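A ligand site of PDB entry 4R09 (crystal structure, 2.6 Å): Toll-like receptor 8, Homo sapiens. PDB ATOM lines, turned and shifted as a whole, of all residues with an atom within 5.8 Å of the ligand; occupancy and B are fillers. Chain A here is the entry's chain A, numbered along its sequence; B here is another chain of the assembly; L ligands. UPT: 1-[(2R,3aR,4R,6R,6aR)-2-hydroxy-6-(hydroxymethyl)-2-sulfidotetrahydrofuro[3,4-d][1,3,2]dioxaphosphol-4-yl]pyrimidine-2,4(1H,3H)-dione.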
ATOM      1  N   ARG A 237      17.218 -19.509   0.716  1.00  0.00           N
ATOM      2  CA  ARG A 237      17.178 -19.047  -0.662  1.00  0.00           C
ATOM      3  C   ARG A 237      17.541 -20.246  -1.549  1.00  0.00           C
ATOM      4  O   ARG A 237      18.663 -20.635  -1.572  1.00  0.00           O
ATOM      5  CB  ARG A 237      18.185 -17.910  -0.851  1.00  0.00           C
ATOM      6  CG  ARG A 237      18.701 -17.750  -2.282  1.00  0.00           C
ATOM      7  CD  ARG A 237      19.717 -16.627  -2.423  1.00  0.00           C
ATOM      8  NE  ARG A 237      20.035 -16.403  -3.829  1.00  0.00           N
ATOM      9  CZ  ARG A 237      20.506 -15.281  -4.345  1.00  0.00           C
ATOM     10  NH1 ARG A 237      20.754 -14.242  -3.606  1.00  0.00           N
ATOM     11  NH2 ARG A 237      20.756 -15.211  -5.631  1.00  0.00           N
ATOM     12  N   ASN A 240      19.216 -22.491  -7.260  1.00  0.00           N
ATOM     13  CA  ASN A 240      20.524 -23.045  -7.550  1.00  0.00           C
ATOM     14  C   ASN A 240      21.116 -23.681  -6.310  1.00  0.00           C
ATOM     15  O   ASN A 240      22.343 -23.707  -6.133  1.00  0.00           O
ATOM     16  CB  ASN A 240      21.461 -21.980  -8.150  1.00  0.00           C
ATOM     17  CG  ASN A 240      22.653 -22.599  -8.845  1.00  0.00           C
ATOM     18  OD1 ASN A 240      22.503 -23.465  -9.707  1.00  0.00           O
ATOM     19  ND2 ASN A 240      23.860 -22.160  -8.470  1.00  0.00           N
ATOM     20  N   ALA A 241      20.227 -24.209  -5.480  1.00  0.00           N
ATOM     21  CA  ALA A 241      20.642 -24.899  -4.285  1.00  0.00           C
ATOM     22  C   ALA A 241      21.432 -26.156  -4.654  1.00  0.00           C
ATOM     23  O   ALA A 241      20.965 -26.975  -5.463  1.00  0.00           O
ATOM     24  CB  ALA A 241      19.431 -25.267  -3.469  1.00  0.00           C
ATOM     25  N   PRO A 242      22.605 -26.341  -4.047  1.00  0.00           N
ATOM     26  CA  PRO A 242      23.346 -27.600  -4.137  1.00  0.00           C
ATOM     27  C   PRO A 242      22.864 -28.723  -3.204  1.00  0.00           C
ATOM     28  O   PRO A 242      23.619 -29.689  -2.931  1.00  0.00           O
ATOM     29  CB  PRO A 242      24.784 -27.181  -3.798  1.00  0.00           C
ATOM     30  CG  PRO A 242      24.649 -25.933  -3.016  1.00  0.00           C
ATOM     31  CD  PRO A 242      23.303 -25.319  -3.263  1.00  0.00           C
ATOM     32  N   PHE A 243      21.596 -28.647  -2.805  1.00  0.00           N
ATOM     33  CA  PHE A 243      20.933 -29.695  -2.003  1.00  0.00           C
ATOM     34  C   PHE A 243      19.409 -29.533  -2.168  1.00  0.00           C
ATOM     35  O   PHE A 243      18.956 -28.477  -2.599  1.00  0.00           O
ATOM     36  CB  PHE A 243      21.311 -29.530  -0.532  1.00  0.00           C
ATOM     37  CG  PHE A 243      21.227 -28.117  -0.077  1.00  0.00           C
ATOM     38  CD1 PHE A 243      20.088 -27.645   0.557  1.00  0.00           C
ATOM     39  CD2 PHE A 243      22.258 -27.213  -0.344  1.00  0.00           C
ATOM     40  CE1 PHE A 243      19.977 -26.319   0.931  1.00  0.00           C
ATOM     41  CE2 PHE A 243      22.156 -25.896   0.050  1.00  0.00           C
ATOM     42  CZ  PHE A 243      21.006 -25.437   0.646  1.00  0.00           C
ATOM     43  N   SER A 274      21.154 -17.477   4.296  1.00  0.00           N
ATOM     44  CA  SER A 274      20.090 -18.237   3.666  1.00  0.00           C
ATOM     45  C   SER A 274      18.870 -18.274   4.521  1.00  0.00           C
ATOM     46  O   SER A 274      18.298 -19.310   4.769  1.00  0.00           O
ATOM     47  CB  SER A 274      20.565 -19.646   3.344  1.00  0.00           C
ATOM     48  OG  SER A 274      19.773 -20.190   2.312  1.00  0.00           O
ATOM     49  N   PHE A 298      23.811 -15.558   0.989  1.00  0.00           N
ATOM     50  CA  PHE A 298      22.628 -16.215   0.366  1.00  0.00           C
ATOM     51  C   PHE A 298      21.292 -15.644   0.888  1.00  0.00           C
ATOM     52  O   PHE A 298      20.387 -16.378   1.306  1.00  0.00           O
ATOM     53  CB  PHE A 298      22.685 -17.736   0.573  1.00  0.00           C
ATOM     54  CG  PHE A 298      23.880 -18.382  -0.090  1.00  0.00           C
ATOM     55  CD1 PHE A 298      23.859 -18.669  -1.431  1.00  0.00           C
ATOM     56  CD2 PHE A 298      24.996 -18.727   0.642  1.00  0.00           C
ATOM     57  CE1 PHE A 298      24.945 -19.281  -2.051  1.00  0.00           C
ATOM     58  CE2 PHE A 298      26.082 -19.331   0.046  1.00  0.00           C
ATOM     59  CZ  PHE A 298      26.057 -19.607  -1.307  1.00  0.00           C
ATOM     60  N   PHE A 324      27.079 -13.989  -1.938  1.00  0.00           N
ATOM     61  CA  PHE A 324      25.956 -14.520  -2.680  1.00  0.00           C
ATOM     62  C   PHE A 324      24.550 -13.897  -2.389  1.00  0.00           C
ATOM     63  O   PHE A 324      23.609 -14.591  -2.059  1.00  0.00           O
ATOM     64  CB  PHE A 324      25.963 -16.037  -2.539  1.00  0.00           C
ATOM     65  CG  PHE A 324      27.011 -16.686  -3.375  1.00  0.00           C
ATOM     66  CD1 PHE A 324      26.871 -16.746  -4.744  1.00  0.00           C
ATOM     67  CD2 PHE A 324      28.158 -17.212  -2.803  1.00  0.00           C
ATOM     68  CE1 PHE A 324      27.835 -17.348  -5.532  1.00  0.00           C
ATOM     69  CE2 PHE A 324      29.148 -17.786  -3.592  1.00  0.00           C
ATOM     70  CZ  PHE A 324      28.984 -17.849  -4.956  1.00  0.00           C
ATOM     71  N   ARG A 353      31.688 -12.428  -1.861  1.00  0.00           N
ATOM     72  CA  ARG A 353      31.661 -13.375  -3.006  1.00  0.00           C
ATOM     73  C   ARG A 353      30.329 -13.176  -3.717  1.00  0.00           C
ATOM     74  O   ARG A 353      29.358 -12.852  -3.073  1.00  0.00           O
ATOM     75  CB  ARG A 353      31.740 -14.832  -2.591  1.00  0.00           C
ATOM     76  CG  ARG A 353      32.998 -15.299  -1.889  1.00  0.00           C
ATOM     77  CD  ARG A 353      32.787 -16.742  -1.406  1.00  0.00           C
ATOM     78  NE  ARG A 353      32.113 -16.689  -0.137  1.00  0.00           N
ATOM     79  CZ  ARG A 353      31.013 -17.340   0.209  1.00  0.00           C
ATOM     80  NH1 ARG A 353      30.442 -18.225  -0.581  1.00  0.00           N
ATOM     81  NH2 ARG A 353      30.517 -17.131   1.391  1.00  0.00           N
ATOM     82  N   ILE A 381      34.390 -14.632  -7.470  1.00  0.00           N
ATOM     83  CA  ILE A 381      33.182 -15.161  -8.100  1.00  0.00           C
ATOM     84  C   ILE A 381      32.164 -14.055  -8.259  1.00  0.00           C
ATOM     85  O   ILE A 381      31.039 -14.211  -7.860  1.00  0.00           O
ATOM     86  CB  ILE A 381      32.588 -16.375  -7.325  1.00  0.00           C
ATOM     87  CG1 ILE A 381      33.691 -17.333  -6.877  1.00  0.00           C
ATOM     88  CG2 ILE A 381      31.608 -17.168  -8.173  1.00  0.00           C
ATOM     89  CD1 ILE A 381      33.249 -18.268  -5.786  1.00  0.00           C
ATOM     90  N   ASN A 444      31.507 -25.277   8.345  1.00  0.00           N
ATOM     91  CA  ASN A 444      30.599 -24.279   7.869  1.00  0.00           C
ATOM     92  C   ASN A 444      29.947 -24.766   6.565  1.00  0.00           C
ATOM     93  O   ASN A 444      30.602 -25.397   5.745  1.00  0.00           O
ATOM     94  CB  ASN A 444      31.348 -22.982   7.619  1.00  0.00           C
ATOM     95  CG  ASN A 444      30.443 -21.774   7.628  1.00  0.00           C
ATOM     96  OD1 ASN A 444      29.624 -21.591   6.749  1.00  0.00           O
ATOM     97  ND2 ASN A 444      30.610 -20.952   8.605  1.00  0.00           N
ATOM     98  N   PHE A 445      28.685 -24.454   6.382  1.00  0.00           N
ATOM     99  CA  PHE A 445      27.896 -24.985   5.280  1.00  0.00           C
ATOM    100  C   PHE A 445      27.710 -23.962   4.128  1.00  0.00           C
ATOM    101  O   PHE A 445      27.236 -24.326   3.027  1.00  0.00           O
ATOM    102  CB  PHE A 445      26.568 -25.436   5.875  1.00  0.00           C
ATOM    103  CG  PHE A 445      25.607 -26.047   4.910  1.00  0.00           C
ATOM    104  CD1 PHE A 445      25.576 -27.429   4.722  1.00  0.00           C
ATOM    105  CD2 PHE A 445      24.621 -25.266   4.313  1.00  0.00           C
ATOM    106  CE1 PHE A 445      24.661 -27.994   3.875  1.00  0.00           C
ATOM    107  CE2 PHE A 445      23.693 -25.849   3.455  1.00  0.00           C
ATOM    108  CZ  PHE A 445      23.705 -27.213   3.243  1.00  0.00           C
ATOM    109  N   TYR A 446      28.073 -22.689   4.346  1.00  0.00           N
ATOM    110  CA  TYR A 446      27.808 -21.654   3.337  1.00  0.00           C
ATOM    111  C   TYR A 446      29.077 -21.050   2.817  1.00  0.00           C
ATOM    112  O   TYR A 446      29.025 -20.305   1.850  1.00  0.00           O
ATOM    113  CB  TYR A 446      26.885 -20.553   3.886  1.00  0.00           C
ATOM    114  CG  TYR A 446      25.517 -21.075   4.251  1.00  0.00           C
ATOM    115  CD1 TYR A 446      24.580 -21.396   3.261  1.00  0.00           C
ATOM    116  CD2 TYR A 446      25.163 -21.284   5.565  1.00  0.00           C
ATOM    117  CE1 TYR A 446      23.335 -21.920   3.587  1.00  0.00           C
ATOM    118  CE2 TYR A 446      23.897 -21.774   5.896  1.00  0.00           C
ATOM    119  CZ  TYR A 446      22.997 -22.079   4.874  1.00  0.00           C
ATOM    120  OH  TYR A 446      21.789 -22.585   5.155  1.00  0.00           O
ATOM    121  N   HIS A 447      30.211 -21.354   3.436  1.00  0.00           N
ATOM    122  CA  HIS A 447      31.501 -21.107   2.788  1.00  0.00           C
ATOM    123  C   HIS A 447      32.587 -22.080   3.189  1.00  0.00           C
ATOM    124  O   HIS A 447      32.456 -22.786   4.177  1.00  0.00           O
ATOM    125  CB  HIS A 447      31.977 -19.658   3.000  1.00  0.00           C
ATOM    126  CG  HIS A 447      32.085 -19.263   4.436  1.00  0.00           C
ATOM    127  ND1 HIS A 447      31.009 -18.776   5.148  1.00  0.00           N
ATOM    128  CD2 HIS A 447      33.140 -19.248   5.275  1.00  0.00           C
ATOM    129  CE1 HIS A 447      31.390 -18.514   6.384  1.00  0.00           C
ATOM    130  NE2 HIS A 447      32.674 -18.788   6.490  1.00  0.00           N
ATOM    131  N   PHE A 448      33.637 -22.139   2.360  1.00  0.00           N
ATOM    132  CA  PHE A 448      34.848 -22.875   2.716  1.00  0.00           C
ATOM    133  C   PHE A 448      35.636 -22.031   3.702  1.00  0.00           C
ATOM    134  O   PHE A 448      35.674 -20.820   3.579  1.00  0.00           O
ATOM    135  CB  PHE A 448      35.718 -23.147   1.495  1.00  0.00           C
ATOM    136  CG  PHE A 448      35.087 -24.056   0.475  1.00  0.00           C
ATOM    137  CD1 PHE A 448      34.781 -25.377   0.790  1.00  0.00           C
ATOM    138  CD2 PHE A 448      34.795 -23.596  -0.806  1.00  0.00           C
ATOM    139  CE1 PHE A 448      34.194 -26.213  -0.143  1.00  0.00           C
ATOM    140  CE2 PHE A 448      34.202 -24.437  -1.732  1.00  0.00           C
ATOM    141  CZ  PHE A 448      33.897 -25.737  -1.399  1.00  0.00           C
ATOM    142  N   ILE B 548      32.150 -25.213  -9.133  1.00  0.00           N
ATOM    143  CA  ILE B 548      31.679 -24.147  -8.268  1.00  0.00           C
ATOM    144  C   ILE B 548      30.156 -24.196  -8.054  1.00  0.00           C
ATOM    145  O   ILE B 548      29.362 -23.779  -8.904  1.00  0.00           O
ATOM    146  CB  ILE B 548      32.061 -22.782  -8.867  1.00  0.00           C
ATOM    147  CG1 ILE B 548      33.592 -22.699  -9.110  1.00  0.00           C
ATOM    148  CG2 ILE B 548      31.621 -21.667  -7.963  1.00  0.00           C
ATOM    149  CD1 ILE B 548      34.002 -21.494  -9.938  1.00  0.00           C
ATOM    150  N   ALA B 549      29.774 -24.647  -6.880  1.00  0.00           N
ATOM    151  CA  ALA B 549      28.392 -24.793  -6.562  1.00  0.00           C
ATOM    152  C   ALA B 549      27.584 -23.514  -6.709  1.00  0.00           C
ATOM    153  O   ALA B 549      26.415 -23.553  -7.075  1.00  0.00           O
ATOM    154  CB  ALA B 549      28.238 -25.352  -5.167  1.00  0.00           C
ATOM    155  N   GLY B 550      28.182 -22.383  -6.405  1.00  0.00           N
ATOM    156  CA  GLY B 550      27.409 -21.136  -6.211  1.00  0.00           C
ATOM    157  C   GLY B 550      26.940 -20.488  -7.494  1.00  0.00           C
ATOM    158  O   GLY B 550      26.008 -19.678  -7.466  1.00  0.00           O
ATOM    159  N   VAL B 551      27.630 -20.804  -8.609  1.00  0.00           N
ATOM    160  CA  VAL B 551      27.250 -20.295  -9.942  1.00  0.00           C
ATOM    161  C   VAL B 551      26.312 -21.260 -10.669  1.00  0.00           C
ATOM    162  O   VAL B 551      26.200 -22.447 -10.307  1.00  0.00           O
ATOM    163  CB  VAL B 551      28.480 -20.021 -10.847  1.00  0.00           C
ATOM    164  CG1 VAL B 551      29.387 -18.975 -10.237  1.00  0.00           C
ATOM    165  CG2 VAL B 551      29.259 -21.298 -11.126  1.00  0.00           C
ATOM    166  N   TYR B 575      28.218 -32.187 -10.535  1.00  0.00           N
ATOM    167  CA  TYR B 575      27.568 -32.649  -9.351  1.00  0.00           C
ATOM    168  C   TYR B 575      26.359 -31.840  -8.953  1.00  0.00           C
ATOM    169  O   TYR B 575      25.686 -32.173  -8.007  1.00  0.00           O
ATOM    170  CB  TYR B 575      28.556 -32.651  -8.216  1.00  0.00           C
ATOM    171  CG  TYR B 575      28.917 -31.292  -7.651  1.00  0.00           C
ATOM    172  CD1 TYR B 575      29.851 -30.485  -8.278  1.00  0.00           C
ATOM    173  CD2 TYR B 575      28.413 -30.867  -6.437  1.00  0.00           C
ATOM    174  CE1 TYR B 575      30.230 -29.265  -7.737  1.00  0.00           C
ATOM    175  CE2 TYR B 575      28.786 -29.652  -5.891  1.00  0.00           C
ATOM    176  CZ  TYR B 575      29.713 -28.871  -6.529  1.00  0.00           C
ATOM    177  OH  TYR B 575      30.080 -27.666  -6.014  1.00  0.00           O
HETATM  178  S   UPT L   1      30.790 -21.069  -4.674  1.00  0.00           S
HETATM  179  P   UPT L   1      31.087 -21.114  -2.778  1.00  0.00           P
HETATM  180  O   UPT L   1      31.446 -22.593  -2.269  1.00  0.00           O
HETATM  181  O5  UPT L   1      32.202 -20.025  -2.395  1.00  0.00           O
HETATM  182  O6  UPT L   1      29.730 -20.999  -1.994  1.00  0.00           O
HETATM  183  C1  UPT L   1      29.396 -22.138  -1.216  1.00  0.00           C
HETATM  184  C2  UPT L   1      30.648 -22.981  -1.151  1.00  0.00           C
HETATM  185  C3  UPT L   1      30.184 -24.427  -1.182  1.00  0.00           C
HETATM  186  C4  UPT L   1      30.282 -25.111   0.179  1.00  0.00           C
HETATM  187  O2  UPT L   1      29.795 -24.294   1.293  1.00  0.00           O
HETATM  188  O1  UPT L   1      28.808 -24.402  -1.632  1.00  0.00           O
HETATM  189  C   UPT L   1      28.374 -23.046  -1.871  1.00  0.00           C
HETATM  190  N   UPT L   1      26.996 -22.926  -1.354  1.00  0.00           N
HETATM  191  C8  UPT L   1      25.905 -22.661  -2.222  1.00  0.00           C
HETATM  192  O4  UPT L   1      26.100 -22.461  -3.429  1.00  0.00           O
HETATM  193  N1  UPT L   1      24.646 -22.610  -1.785  1.00  0.00           N
HETATM  194  C7  UPT L   1      24.393 -22.848  -0.486  1.00  0.00           C
HETATM  195  O3  UPT L   1      23.224 -22.763  -0.060  1.00  0.00           O
HETATM  196  C5  UPT L   1      25.422 -23.161   0.378  1.00  0.00           C
HETATM  197  C6  UPT L   1      26.730 -23.190  -0.089  1.00  0.00           C
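CD of Pro 242 touches N1 of the ligand, at 3.4 Å. Phe 243 touches the ligand (CE2 to O3, 3.3 Å). CZ of Phe 298 touches C8 of the ligand (3.2 Å). CE2 of Phe 324 touches O6 of the ligand (3.6 Å). CD1 of Ile 381 touches S of the ligand (3.9 Å). Tyr 446 touches the ligand. His 447 touches the ligand. Phe 448 touches the ligand. Ile 548 of chain B touches the ligand (CG2 to S, 3.4 Å). Ala 549 of chain B touches the ligand (CB to O1, 3.7 Å). 13 residues have an atom within 4 Å of the ligand: Pro 242, Phe 243, Phe 298, Phe 324, Arg 353, Ile 381, Phe 445, Tyr 446, His 447, Phe 448, Ile 548 of chain B, Ala 549 of chain B and Gly 550 of chain B.
N of Phe 298 sits close to O of Phe 324, at 3.2 Å. The guanidinium group of Arg 237 is in hydrogen-bond range of the backbone carbonyl oxygen of Phe 324, at 3.3 Å. O of Ala 549 of chain B is in hydrogen-bond range of ND2 of Asn 240, at 3.2 Å. The backbone carbonyl oxygen (O) of Tyr 446 lies within hydrogen-bond range of the guanidinium group (NH1) of Arg 353, 3.5 Å away. O of Arg 353 is in hydrogen-bond range of N of Phe 324 (2.8 Å). The backbone carbonyl oxygen (O) of Phe 298 sits close to the backbone NH (N) of Ser 274, at 3.3 Å. OD1 of Asn 444 sits at hydrogen-bond distance from N of Tyr 446, 3.1 Å away. The backbone NH of His 447 is in hydrogen-bond range of the side-chain amide oxygen of Asn 444 (3.4 Å).
N of Gly 550 of chain B lies close to S of the ligand, at 3.4 Å. The backbone carbonyl oxygen (O) of Phe 445 lies within hydrogen-bond range of an oxygen (O2) of the ligand (3.1 Å). O5 of the ligand lies within hydrogen-bond range of NH1 of Arg 353, 3.1 Å away.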
